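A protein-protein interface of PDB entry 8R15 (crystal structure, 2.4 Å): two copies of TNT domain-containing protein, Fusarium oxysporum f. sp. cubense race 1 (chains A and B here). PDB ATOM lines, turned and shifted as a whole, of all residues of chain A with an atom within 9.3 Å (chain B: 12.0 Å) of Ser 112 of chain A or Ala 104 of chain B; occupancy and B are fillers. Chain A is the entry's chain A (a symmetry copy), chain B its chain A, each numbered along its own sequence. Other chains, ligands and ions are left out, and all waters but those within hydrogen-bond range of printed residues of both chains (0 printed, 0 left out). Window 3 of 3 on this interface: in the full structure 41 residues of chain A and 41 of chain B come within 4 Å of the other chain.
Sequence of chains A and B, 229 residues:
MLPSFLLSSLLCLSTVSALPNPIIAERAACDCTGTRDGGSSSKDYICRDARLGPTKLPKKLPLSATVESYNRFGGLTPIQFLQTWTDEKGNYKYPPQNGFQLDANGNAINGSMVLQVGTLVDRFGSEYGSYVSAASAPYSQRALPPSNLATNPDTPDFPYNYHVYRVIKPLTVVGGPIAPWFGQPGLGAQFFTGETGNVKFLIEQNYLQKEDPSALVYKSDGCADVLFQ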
ATOM      1  N   PHE A 100      14.538 -35.399   2.476  1.00  0.00           N
ATOM      2  CA  PHE A 100      15.025 -34.152   1.915  1.00  0.00           C
ATOM      3  C   PHE A 100      14.403 -33.912   0.542  1.00  0.00           C
ATOM      4  O   PHE A 100      14.105 -34.848  -0.207  1.00  0.00           O
ATOM      5  CB  PHE A 100      16.553 -34.173   1.806  1.00  0.00           C
ATOM      6  CG  PHE A 100      17.264 -34.041   3.121  1.00  0.00           C
ATOM      7  CD1 PHE A 100      17.441 -32.799   3.694  1.00  0.00           C
ATOM      8  CD2 PHE A 100      17.750 -35.154   3.782  1.00  0.00           C
ATOM      9  CE1 PHE A 100      18.086 -32.664   4.905  1.00  0.00           C
ATOM     10  CE2 PHE A 100      18.404 -35.029   4.993  1.00  0.00           C
ATOM     11  CZ  PHE A 100      18.578 -33.781   5.556  1.00  0.00           C
ATOM     12  N   ILE A 109      18.760 -32.270  -1.443  1.00  0.00           N
ATOM     13  CA  ILE A 109      19.299 -30.942  -1.188  1.00  0.00           C
ATOM     14  C   ILE A 109      19.616 -30.847   0.306  1.00  0.00           C
ATOM     15  O   ILE A 109      18.710 -30.853   1.146  1.00  0.00           O
ATOM     16  CB  ILE A 109      18.306 -29.863  -1.621  1.00  0.00           C
ATOM     17  CG1 ILE A 109      18.038 -30.004  -3.123  1.00  0.00           C
ATOM     18  CG2 ILE A 109      18.824 -28.485  -1.253  1.00  0.00           C
ATOM     19  CD1 ILE A 109      16.934 -29.148  -3.672  1.00  0.00           C
ATOM     20  N   ASN A 110      20.899 -30.765   0.645  1.00  0.00           N
ATOM     21  CA  ASN A 110      21.299 -30.620   2.032  1.00  0.00           C
ATOM     22  C   ASN A 110      22.726 -30.097   2.074  1.00  0.00           C
ATOM     23  O   ASN A 110      23.344 -29.817   1.043  1.00  0.00           O
ATOM     24  CB  ASN A 110      21.178 -31.945   2.780  1.00  0.00           C
ATOM     25  CG  ASN A 110      22.105 -33.012   2.237  1.00  0.00           C
ATOM     26  OD1 ASN A 110      23.308 -32.789   2.122  1.00  0.00           O
ATOM     27  ND2 ASN A 110      21.560 -34.167   1.893  1.00  0.00           N
ATOM     28  N   GLY A 111      23.252 -29.980   3.294  1.00  0.00           N
ATOM     29  CA  GLY A 111      24.636 -29.577   3.482  1.00  0.00           C
ATOM     30  C   GLY A 111      24.996 -29.419   4.942  1.00  0.00           C
ATOM     31  O   GLY A 111      24.130 -29.131   5.772  1.00  0.00           O
ATOM     32  N   SER A 112      26.266 -29.621   5.264  1.00  0.00           N
ATOM     33  CA  SER A 112      26.737 -29.478   6.634  1.00  0.00           C
ATOM     34  C   SER A 112      26.667 -28.018   7.065  1.00  0.00           C
ATOM     35  O   SER A 112      27.302 -27.152   6.456  1.00  0.00           O
ATOM     36  CB  SER A 112      28.168 -29.999   6.763  1.00  0.00           C
ATOM     37  OG  SER A 112      28.236 -31.417   6.793  1.00  0.00           O
ATOM     38  N   MET A 113      25.911 -27.747   8.129  1.00  0.00           N
ATOM     39  CA  MET A 113      25.770 -26.397   8.652  1.00  0.00           C
ATOM     40  C   MET A 113      25.792 -26.418  10.174  1.00  0.00           C
ATOM     41  O   MET A 113      25.388 -27.398  10.807  1.00  0.00           O
ATOM     42  CB  MET A 113      24.473 -25.752   8.169  1.00  0.00           C
ATOM     43  CG  MET A 113      23.329 -26.734   8.060  1.00  0.00           C
ATOM     44  SD  MET A 113      21.708 -25.939   8.079  1.00  0.00           S
ATOM     45  CE  MET A 113      21.633 -25.383   9.776  1.00  0.00           C
ATOM     46  N   VAL A 114      26.241 -25.309  10.753  1.00  0.00           N
ATOM     47  CA  VAL A 114      26.300 -25.160  12.202  1.00  0.00           C
ATOM     48  C   VAL A 114      25.005 -24.525  12.686  1.00  0.00           C
ATOM     49  O   VAL A 114      24.562 -23.504  12.145  1.00  0.00           O
ATOM     50  CB  VAL A 114      27.516 -24.317  12.624  1.00  0.00           C
ATOM     51  CG1 VAL A 114      27.565 -24.170  14.144  1.00  0.00           C
ATOM     52  CG2 VAL A 114      28.806 -24.941  12.104  1.00  0.00           C
ATOM     53  N   LEU A 115      24.398 -25.129  13.706  1.00  0.00           N
ATOM     54  CA  LEU A 115      23.260 -24.535  14.400  1.00  0.00           C
ATOM     55  C   LEU A 115      23.782 -23.657  15.532  1.00  0.00           C
ATOM     56  O   LEU A 115      24.428 -24.153  16.462  1.00  0.00           O
ATOM     57  CB  LEU A 115      22.314 -25.611  14.940  1.00  0.00           C
ATOM     58  CG  LEU A 115      21.534 -26.475  13.942  1.00  0.00           C
ATOM     59  CD1 LEU A 115      20.903 -27.678  14.636  1.00  0.00           C
ATOM     60  CD2 LEU A 115      20.467 -25.658  13.228  1.00  0.00           C
ATOM     61  N   GLN A 116      23.505 -22.359  15.447  1.00  0.00           N
ATOM     62  CA  GLN A 116      23.969 -21.409  16.447  1.00  0.00           C
ATOM     63  C   GLN A 116      23.270 -21.634  17.781  1.00  0.00           C
ATOM     64  O   GLN A 116      22.142 -22.133  17.843  1.00  0.00           O
ATOM     65  CB  GLN A 116      23.725 -19.979  15.971  1.00  0.00           C
ATOM     66  CG  GLN A 116      24.936 -19.343  15.299  1.00  0.00           C
ATOM     67  CD  GLN A 116      25.422 -20.131  14.100  1.00  0.00           C
ATOM     68  OE1 GLN A 116      24.840 -20.057  13.013  1.00  0.00           O
ATOM     69  NE2 GLN A 116      26.497 -20.892  14.288  1.00  0.00           N
ATOM     70  N   LEU A 171      26.192 -26.938  17.169  1.00  0.00           N
ATOM     71  CA  LEU A 171      26.096 -28.300  16.666  1.00  0.00           C
ATOM     72  C   LEU A 171      26.043 -28.249  15.145  1.00  0.00           C
ATOM     73  O   LEU A 171      25.092 -27.711  14.568  1.00  0.00           O
ATOM     74  CB  LEU A 171      24.866 -28.998  17.238  1.00  0.00           C
ATOM     75  CG  LEU A 171      24.531 -30.342  16.608  1.00  0.00           C
ATOM     76  CD1 LEU A 171      25.486 -31.399  17.120  1.00  0.00           C
ATOM     77  CD2 LEU A 171      23.093 -30.699  16.927  1.00  0.00           C
ATOM     78  N   THR A 172      27.057 -28.807  14.497  1.00  0.00           N
ATOM     79  CA  THR A 172      27.019 -28.947  13.052  1.00  0.00           C
ATOM     80  C   THR A 172      26.076 -30.084  12.678  1.00  0.00           C
ATOM     81  O   THR A 172      26.123 -31.163  13.276  1.00  0.00           O
ATOM     82  CB  THR A 172      28.424 -29.207  12.513  1.00  0.00           C
ATOM     83  OG1 THR A 172      29.346 -28.310  13.144  1.00  0.00           O
ATOM     84  CG2 THR A 172      28.463 -28.974  11.012  1.00  0.00           C
ATOM     85  N   VAL A 173      25.206 -29.846  11.696  1.00  0.00           N
ATOM     86  CA  VAL A 173      24.274 -30.860  11.218  1.00  0.00           C
ATOM     87  C   VAL A 173      24.220 -30.778   9.704  1.00  0.00           C
ATOM     88  O   VAL A 173      24.647 -29.794   9.101  1.00  0.00           O
ATOM     89  CB  VAL A 173      22.857 -30.671  11.791  1.00  0.00           C
ATOM     90  CG1 VAL A 173      22.850 -30.864  13.297  1.00  0.00           C
ATOM     91  CG2 VAL A 173      22.333 -29.303  11.430  1.00  0.00           C
ATOM     92  N   VAL A 174      23.672 -31.819   9.085  1.00  0.00           N
ATOM     93  CA  VAL A 174      23.389 -31.776   7.655  1.00  0.00           C
ATOM     94  C   VAL A 174      21.913 -31.408   7.535  1.00  0.00           C
ATOM     95  O   VAL A 174      21.019 -32.201   7.845  1.00  0.00           O
ATOM     96  CB  VAL A 174      23.755 -33.085   6.952  1.00  0.00           C
ATOM     97  CG1 VAL A 174      23.377 -34.283   7.784  1.00  0.00           C
ATOM     98  CG2 VAL A 174      23.131 -33.150   5.566  1.00  0.00           C
ATOM     99  N   GLY A 175      21.661 -30.174   7.109  1.00  0.00           N
ATOM    100  CA  GLY A 175      20.327 -29.607   7.087  1.00  0.00           C
ATOM    101  C   GLY A 175      19.860 -29.333   5.673  1.00  0.00           C
ATOM    102  O   GLY A 175      20.668 -29.088   4.777  1.00  0.00           O
ATOM    103  N   GLY A 176      18.546 -29.398   5.471  1.00  0.00           N
ATOM    104  CA  GLY A 176      17.974 -29.157   4.170  1.00  0.00           C
ATOM    105  C   GLY A 176      16.470 -28.977   4.203  1.00  0.00           C
ATOM    106  O   GLY A 176      15.817 -29.133   5.237  1.00  0.00           O
ATOM    107  N   PHE A 191      17.060 -31.327  10.074  1.00  0.00           N
ATOM    108  CA  PHE A 191      18.488 -31.428  10.357  1.00  0.00           C
ATOM    109  C   PHE A 191      18.803 -32.822  10.861  1.00  0.00           C
ATOM    110  O   PHE A 191      18.262 -33.241  11.888  1.00  0.00           O
ATOM    111  CB  PHE A 191      18.923 -30.393  11.396  1.00  0.00           C
ATOM    112  CG  PHE A 191      18.404 -29.017  11.123  1.00  0.00           C
ATOM    113  CD1 PHE A 191      18.953 -28.240  10.112  1.00  0.00           C
ATOM    114  CD2 PHE A 191      17.364 -28.505  11.868  1.00  0.00           C
ATOM    115  CE1 PHE A 191      18.471 -26.988   9.854  1.00  0.00           C
ATOM    116  CE2 PHE A 191      16.873 -27.237  11.614  1.00  0.00           C
ATOM    117  CZ  PHE A 191      17.430 -26.480  10.608  1.00  0.00           C
ATOM    118  N   PHE A 192      19.671 -33.528  10.143  1.00  0.00           N
ATOM    119  CA  PHE A 192      20.184 -34.827  10.566  1.00  0.00           C
ATOM    120  C   PHE A 192      21.353 -34.604  11.520  1.00  0.00           C
ATOM    121  O   PHE A 192      22.319 -33.911  11.180  1.00  0.00           O
ATOM    122  CB  PHE A 192      20.615 -35.641   9.346  1.00  0.00           C
ATOM    123  CG  PHE A 192      21.274 -36.970   9.663  1.00  0.00           C
ATOM    124  CD1 PHE A 192      20.597 -37.959  10.361  1.00  0.00           C
ATOM    125  CD2 PHE A 192      22.556 -37.251   9.198  1.00  0.00           C
ATOM    126  CE1 PHE A 192      21.202 -39.184  10.621  1.00  0.00           C
ATOM    127  CE2 PHE A 192      23.160 -38.472   9.454  1.00  0.00           C
ATOM    128  CZ  PHE A 192      22.481 -39.435  10.164  1.00  0.00           C
ATOM    129  N   GLU A 195      25.670 -37.429  12.399  1.00  0.00           N
ATOM    130  CA  GLU A 195      27.116 -37.293  12.275  1.00  0.00           C
ATOM    131  C   GLU A 195      27.759 -37.101  13.637  1.00  0.00           C
ATOM    132  O   GLU A 195      28.892 -37.546  13.863  1.00  0.00           O
ATOM    133  CB  GLU A 195      27.456 -36.127  11.343  1.00  0.00           C
ATOM    134  CG  GLU A 195      28.623 -36.392  10.409  1.00  0.00           C
ATOM    135  CD  GLU A 195      28.248 -37.318   9.262  1.00  0.00           C
ATOM    136  OE1 GLU A 195      27.053 -37.335   8.890  1.00  0.00           O
ATOM    137  OE2 GLU A 195      29.144 -38.027   8.741  1.00  0.00           O
ATOM    138  N   THR A 196      27.052 -36.450  14.557  1.00  0.00           N
ATOM    139  CA  THR A 196      27.482 -36.337  15.943  1.00  0.00           C
ATOM    140  C   THR A 196      26.855 -37.410  16.822  1.00  0.00           C
ATOM    141  O   THR A 196      27.568 -38.179  17.472  1.00  0.00           O
ATOM    142  CB  THR A 196      27.121 -34.961  16.500  1.00  0.00           C
ATOM    143  OG1 THR A 196      27.618 -33.940  15.625  1.00  0.00           O
ATOM    144  CG2 THR A 196      27.716 -34.785  17.878  1.00  0.00           C
ATOM    145  N   GLN B  97      25.488 -13.963   0.292  1.00  0.00           N
ATOM    146  CA  GLN B  97      25.113 -15.024  -0.645  1.00  0.00           C
ATOM    147  C   GLN B  97      23.598 -15.201  -0.705  1.00  0.00           C
ATOM    148  O   GLN B  97      23.063 -16.299  -0.528  1.00  0.00           O
ATOM    149  CB  GLN B  97      25.806 -16.337  -0.288  1.00  0.00           C
ATOM    150  CG  GLN B  97      27.319 -16.215  -0.252  1.00  0.00           C
ATOM    151  CD  GLN B  97      27.997 -17.512   0.114  1.00  0.00           C
ATOM    152  OE1 GLN B  97      27.785 -18.543  -0.530  1.00  0.00           O
ATOM    153  NE2 GLN B  97      28.813 -17.474   1.161  1.00  0.00           N
ATOM    154  N   PHE B 100      20.872 -17.338   1.681  1.00  0.00           N
ATOM    155  CA  PHE B 100      20.867 -18.768   1.933  1.00  0.00           C
ATOM    156  C   PHE B 100      21.705 -19.090   3.168  1.00  0.00           C
ATOM    157  O   PHE B 100      22.694 -18.416   3.473  1.00  0.00           O
ATOM    158  CB  PHE B 100      21.404 -19.530   0.717  1.00  0.00           C
ATOM    159  CG  PHE B 100      20.457 -19.572  -0.447  1.00  0.00           C
ATOM    160  CD1 PHE B 100      19.431 -20.492  -0.474  1.00  0.00           C
ATOM    161  CD2 PHE B 100      20.595 -18.696  -1.507  1.00  0.00           C
ATOM    162  CE1 PHE B 100      18.550 -20.537  -1.535  1.00  0.00           C
ATOM    163  CE2 PHE B 100      19.721 -18.737  -2.578  1.00  0.00           C
ATOM    164  CZ  PHE B 100      18.698 -19.663  -2.595  1.00  0.00           C
ATOM    165  N   GLN B 101      21.295 -20.133   3.883  1.00  0.00           N
ATOM    166  CA  GLN B 101      22.129 -20.681   4.940  1.00  0.00           C
ATOM    167  C   GLN B 101      23.436 -21.187   4.342  1.00  0.00           C
ATOM    168  O   GLN B 101      23.433 -21.961   3.379  1.00  0.00           O
ATOM    169  CB  GLN B 101      21.388 -21.808   5.658  1.00  0.00           C
ATOM    170  CG  GLN B 101      22.247 -22.614   6.619  1.00  0.00           C
ATOM    171  CD  GLN B 101      22.681 -21.813   7.830  1.00  0.00           C
ATOM    172  OE1 GLN B 101      21.889 -21.083   8.415  1.00  0.00           O
ATOM    173  NE2 GLN B 101      23.942 -21.945   8.209  1.00  0.00           N
ATOM    174  N   LEU B 102      24.554 -20.731   4.900  1.00  0.00           N
ATOM    175  CA  LEU B 102      25.872 -21.109   4.410  1.00  0.00           C
ATOM    176  C   LEU B 102      26.343 -22.387   5.093  1.00  0.00           C
ATOM    177  O   LEU B 102      26.183 -22.552   6.306  1.00  0.00           O
ATOM    178  CB  LEU B 102      26.886 -19.988   4.652  1.00  0.00           C
ATOM    179  CG  LEU B 102      26.438 -18.592   4.224  1.00  0.00           C
ATOM    180  CD1 LEU B 102      27.512 -17.558   4.490  1.00  0.00           C
ATOM    181  CD2 LEU B 102      26.061 -18.608   2.767  1.00  0.00           C
ATOM    182  N   ASP B 103      26.943 -23.283   4.309  1.00  0.00           N
ATOM    183  CA  ASP B 103      27.461 -24.528   4.860  1.00  0.00           C
ATOM    184  C   ASP B 103      28.673 -24.247   5.752  1.00  0.00           C
ATOM    185  O   ASP B 103      29.088 -23.102   5.948  1.00  0.00           O
ATOM    186  CB  ASP B 103      27.785 -25.522   3.737  1.00  0.00           C
ATOM    187  CG  ASP B 103      28.951 -25.083   2.839  1.00  0.00           C
ATOM    188  OD1 ASP B 103      29.588 -24.037   3.088  1.00  0.00           O
ATOM    189  OD2 ASP B 103      29.233 -25.807   1.859  1.00  0.00           O
ATOM    190  N   ALA B 104      29.241 -25.321   6.308  1.00  0.00           N
ATOM    191  CA  ALA B 104      30.428 -25.191   7.148  1.00  0.00           C
ATOM    192  C   ALA B 104      31.591 -24.551   6.400  1.00  0.00           C
ATOM    193  O   ALA B 104      32.366 -23.797   6.999  1.00  0.00           O
ATOM    194  CB  ALA B 104      30.840 -26.561   7.676  1.00  0.00           C
ATOM    195  N   ASN B 105      31.704 -24.800   5.097  1.00  0.00           N
ATOM    196  CA  ASN B 105      32.754 -24.223   4.270  1.00  0.00           C
ATOM    197  C   ASN B 105      32.424 -22.818   3.789  1.00  0.00           C
ATOM    198  O   ASN B 105      33.173 -22.274   2.974  1.00  0.00           O
ATOM    199  CB  ASN B 105      33.030 -25.124   3.063  1.00  0.00           C
ATOM    200  CG  ASN B 105      33.149 -26.583   3.442  1.00  0.00           C
ATOM    201  OD1 ASN B 105      34.131 -26.998   4.060  1.00  0.00           O
ATOM    202  ND2 ASN B 105      32.156 -27.375   3.062  1.00  0.00           N
ATOM    203  N   GLY B 106      31.324 -22.230   4.253  1.00  0.00           N
ATOM    204  CA  GLY B 106      30.967 -20.888   3.846  1.00  0.00           C
ATOM    205  C   GLY B 106      30.240 -20.787   2.527  1.00  0.00           C
ATOM    206  O   GLY B 106      30.128 -19.685   1.981  1.00  0.00           O
ATOM    207  N   ASN B 107      29.735 -21.897   1.998  1.00  0.00           N
ATOM    208  CA  ASN B 107      29.022 -21.912   0.727  1.00  0.00           C
ATOM    209  C   ASN B 107      27.526 -22.101   0.966  1.00  0.00           C
ATOM    210  O   ASN B 107      27.116 -22.918   1.800  1.00  0.00           O
ATOM    211  CB  ASN B 107      29.557 -23.021  -0.183  1.00  0.00           C
ATOM    212  CG  ASN B 107      31.040 -22.883  -0.453  1.00  0.00           C
ATOM    213  OD1 ASN B 107      31.550 -21.776  -0.627  1.00  0.00           O
ATOM    214  ND2 ASN B 107      31.742 -24.009  -0.479  1.00  0.00           N
ATOM    215  N   ALA B 108      26.716 -21.349   0.218  1.00  0.00           N
ATOM    216  CA  ALA B 108      25.272 -21.376   0.406  1.00  0.00           C
ATOM    217  C   ALA B 108      24.716 -22.770   0.161  1.00  0.00           C
ATOM    218  O   ALA B 108      25.094 -23.455  -0.792  1.00  0.00           O
ATOM    219  CB  ALA B 108      24.591 -20.379  -0.533  1.00  0.00           C
ATOM    220  N   ILE B 109      23.788 -23.173   1.020  1.00  0.00           N
ATOM    221  CA  ILE B 109      23.084 -24.438   0.870  1.00  0.00           C
ATOM    222  C   ILE B 109      21.896 -24.204  -0.065  1.00  0.00           C
ATOM    223  O   ILE B 109      20.947 -23.494   0.286  1.00  0.00           O
ATOM    224  CB  ILE B 109      22.632 -24.969   2.232  1.00  0.00           C
ATOM    225  CG1 ILE B 109      23.864 -25.194   3.115  1.00  0.00           C
ATOM    226  CG2 ILE B 109      21.805 -26.230   2.062  1.00  0.00           C
ATOM    227  CD1 ILE B 109      23.583 -25.526   4.552  1.00  0.00           C
ATOM    228  N   ASN B 110      21.943 -24.790  -1.257  1.00  0.00           N
ATOM    229  CA  ASN B 110      20.844 -24.669  -2.194  1.00  0.00           C
ATOM    230  C   ASN B 110      20.961 -25.778  -3.227  1.00  0.00           C
ATOM    231  O   ASN B 110      21.853 -26.629  -3.165  1.00  0.00           O
ATOM    232  CB  ASN B 110      20.837 -23.296  -2.861  1.00  0.00           C
ATOM    233  CG  ASN B 110      22.070 -23.047  -3.704  1.00  0.00           C
ATOM    234  OD1 ASN B 110      22.400 -23.851  -4.573  1.00  0.00           O
ATOM    235  ND2 ASN B 110      22.760 -21.946  -3.454  1.00  0.00           N
ATOM    236  N   GLY B 111      20.049 -25.748  -4.199  1.00  0.00           N
ATOM    237  CA  GLY B 111      20.093 -26.692  -5.304  1.00  0.00           C
ATOM    238  C   GLY B 111      18.914 -26.540  -6.238  1.00  0.00           C
ATOM    239  O   GLY B 111      17.841 -26.093  -5.825  1.00  0.00           O
ATOM    240  N   GLY B 176      16.623 -23.247  -1.159  1.00  0.00           N
ATOM    241  CA  GLY B 176      17.415 -23.573   0.001  1.00  0.00           C
ATOM    242  C   GLY B 176      16.871 -22.977   1.282  1.00  0.00           C
ATOM    243  O   GLY B 176      15.907 -22.207   1.285  1.00  0.00           O
ATOM    244  N   PRO B 177      17.485 -23.331   2.404  1.00  0.00           N
ATOM    245  CA  PRO B 177      17.093 -22.736   3.682  1.00  0.00           C
ATOM    246  C   PRO B 177      17.562 -21.294   3.795  1.00  0.00           C
ATOM    247  O   PRO B 177      18.604 -20.907   3.261  1.00  0.00           O
ATOM    248  CB  PRO B 177      17.796 -23.627   4.711  1.00  0.00           C
ATOM    249  CG  PRO B 177      18.997 -24.137   3.992  1.00  0.00           C
ATOM    250  CD  PRO B 177      18.546 -24.341   2.567  1.00  0.00           C
ATOM    251  N   ALA B 179      19.004 -18.180   5.837  1.00  0.00           N
ATOM    252  CA  ALA B 179      19.901 -18.034   6.974  1.00  0.00           C
ATOM    253  C   ALA B 179      19.272 -17.124   8.026  1.00  0.00           C
ATOM    254  O   ALA B 179      18.601 -16.141   7.681  1.00  0.00           O
ATOM    255  CB  ALA B 179      21.253 -17.476   6.541  1.00  0.00           C
ATOM    256  N   PRO B 180      19.438 -17.440   9.309  1.00  0.00           N
ATOM    257  CA  PRO B 180      18.990 -16.519  10.359  1.00  0.00           C
ATOM    258  C   PRO B 180      19.631 -15.150  10.175  1.00  0.00           C
ATOM    259  O   PRO B 180      20.781 -15.035   9.743  1.00  0.00           O
ATOM    260  CB  PRO B 180      19.464 -17.192  11.651  1.00  0.00           C
ATOM    261  CG  PRO B 180      19.575 -18.643  11.286  1.00  0.00           C
ATOM    262  CD  PRO B 180      20.020 -18.676   9.856  1.00  0.00           C
ATOM    263  N   LEU B 187      15.493 -19.893   8.644  1.00  0.00           N
ATOM    264  CA  LEU B 187      15.410 -21.313   8.308  1.00  0.00           C
ATOM    265  C   LEU B 187      14.147 -21.667   7.531  1.00  0.00           C
ATOM    266  O   LEU B 187      13.809 -22.848   7.402  1.00  0.00           O
ATOM    267  CB  LEU B 187      15.538 -22.197   9.555  1.00  0.00           C
ATOM    268  CG  LEU B 187      16.881 -22.065  10.285  1.00  0.00           C
ATOM    269  CD1 LEU B 187      16.953 -22.956  11.517  1.00  0.00           C
ATOM    270  CD2 LEU B 187      18.036 -22.358   9.331  1.00  0.00           C
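The backbone NH (N) of Ala 104 of chain B lies within hydrogen-bond range of the backbone carbonyl oxygen (O) of Ser 112 of chain A (2.7 Å).
The backbone carbonyl oxygen of Gln 101 of chain B lies within hydrogen-bond range of the backbone NH of Ile 109 of chain B. O of Pro 177 of chain B sits at hydrogen-bond distance from N of Gln 101 of chain B (2.9 Å). The side-chain carboxylate (OD1) of Asp 103 of chain B sits at hydrogen-bond distance from the backbone NH (N) of Asn 105 of chain B (3.0 Å). The backbone NH (N) of Asn 107 of chain B is in hydrogen-bond range of the side-chain carboxylate (OD1) of Asp 103 of chain B. O of Gly 111 of chain A lies within hydrogen-bond range of N of Gly 175 of chain A (3.0 Å). The backbone NH of Met 113 of chain A sits at hydrogen-bond distance from the backbone carbonyl oxygen of Val 173 of chain A (2.6 Å).
Among the printed residues, pairs that only touch across the chains: Ser 112 of chain A with Asp 103 of chain B, Phe 191 of chain A with Leu 187 of chain B, Met 113 of chain A with Gln 101 of chain B, Met 113 of chain A with Ile 109 of chain B, Gly 111 of chain A with Ile 109 of chain B, Ile 109 of chain A with Gly 111 of chain B, Ile 109 of chain A with Asn 110 of chain B and Asn 110 of chain A with Ile 109 of chain B.
Of chain B, only Asp 103 and Ala 104 come within 4 Å of Ser 112 of chain A. Ala 104 of chain B touches just one residue of chain A: Ser 112 (2.7 Å). Printed residues of chain B within 4 Å of Asn 110 of chain A: Ile 109 (3.98 Å). Gly 111 of chain A touches one residue of chain B. No residue of chain B comes within 4 Å of Val 114 of chain A. Thr 172 of chain A touches none of the printed residues of chain B. No residue of chain B comes within 4 Å of Val 173 of chain A. No residue of chain B comes within 4 Å of Val 174 of chain A. No residue of chain A comes within 4 Å of Asn 105 of chain B. Of the printed residues of chain A, Gln 101 of chain B touches Met 113 (3.7 Å). Of the printed residues of chain B, Phe 191 of chain A touches Leu 187. Of the printed residues of chain A, Asn 110 of chain B touches Ile 109 (3.97 Å). Of the printed residues of chain A, Leu 187 of chain B touches Phe 191 (3.7 Å). Gly 176 of chain B touches none of the printed residues of chain A. Phe 100 of chain B touches none of the printed residues of chain A. The nearest residue of chain A that does not touch Ala 104 of chain B is Met 113 of chain A (4.3 Å). The nearest printed residue of chain B that does not touch Ile 109 of chain A is Ile 109 of chain B (5.0 Å).
Of the 19 printed residues of chain A, 6 touch a printed residue of chain B. Hydrophobic or aromatic side chains of chain A that line the printed part of chain B: Ile 109, Met 113 and Phe 191. Printed residues of chain B that touch a printed residue of chain A: Gln 101, Asp 103, Ala 104, Ile 109, Asn 110, Gly 111 and Leu 187. Hydrophobic or aromatic side chains of chain B that line the printed part of chain A: Ala 104, Ile 109 and Leu 187. Along chain B the printed residues that touch a printed residue of chain A span positions 101 to 187. Among the printed residues, 9 pairs touch across the chains. Among the printed residues, no Asp or Glu carboxylate lies within 4 Å of a Lys or Arg side-chain nitrogen of the other chain.
Ile 109 of chain A touches Asn 110 of chain B, and with the chains exchanged Asn 110 of chain A touches Ile 109 of chain B. Ile 109 of chain A touches Gly 111 of chain B, and with the chains exchanged Gly 111 of chain A touches Ile 109 of chain B. Of the 9 pairs that touch across the chains among the printed residues, 4 have their exchanged pair printed and touching as well.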
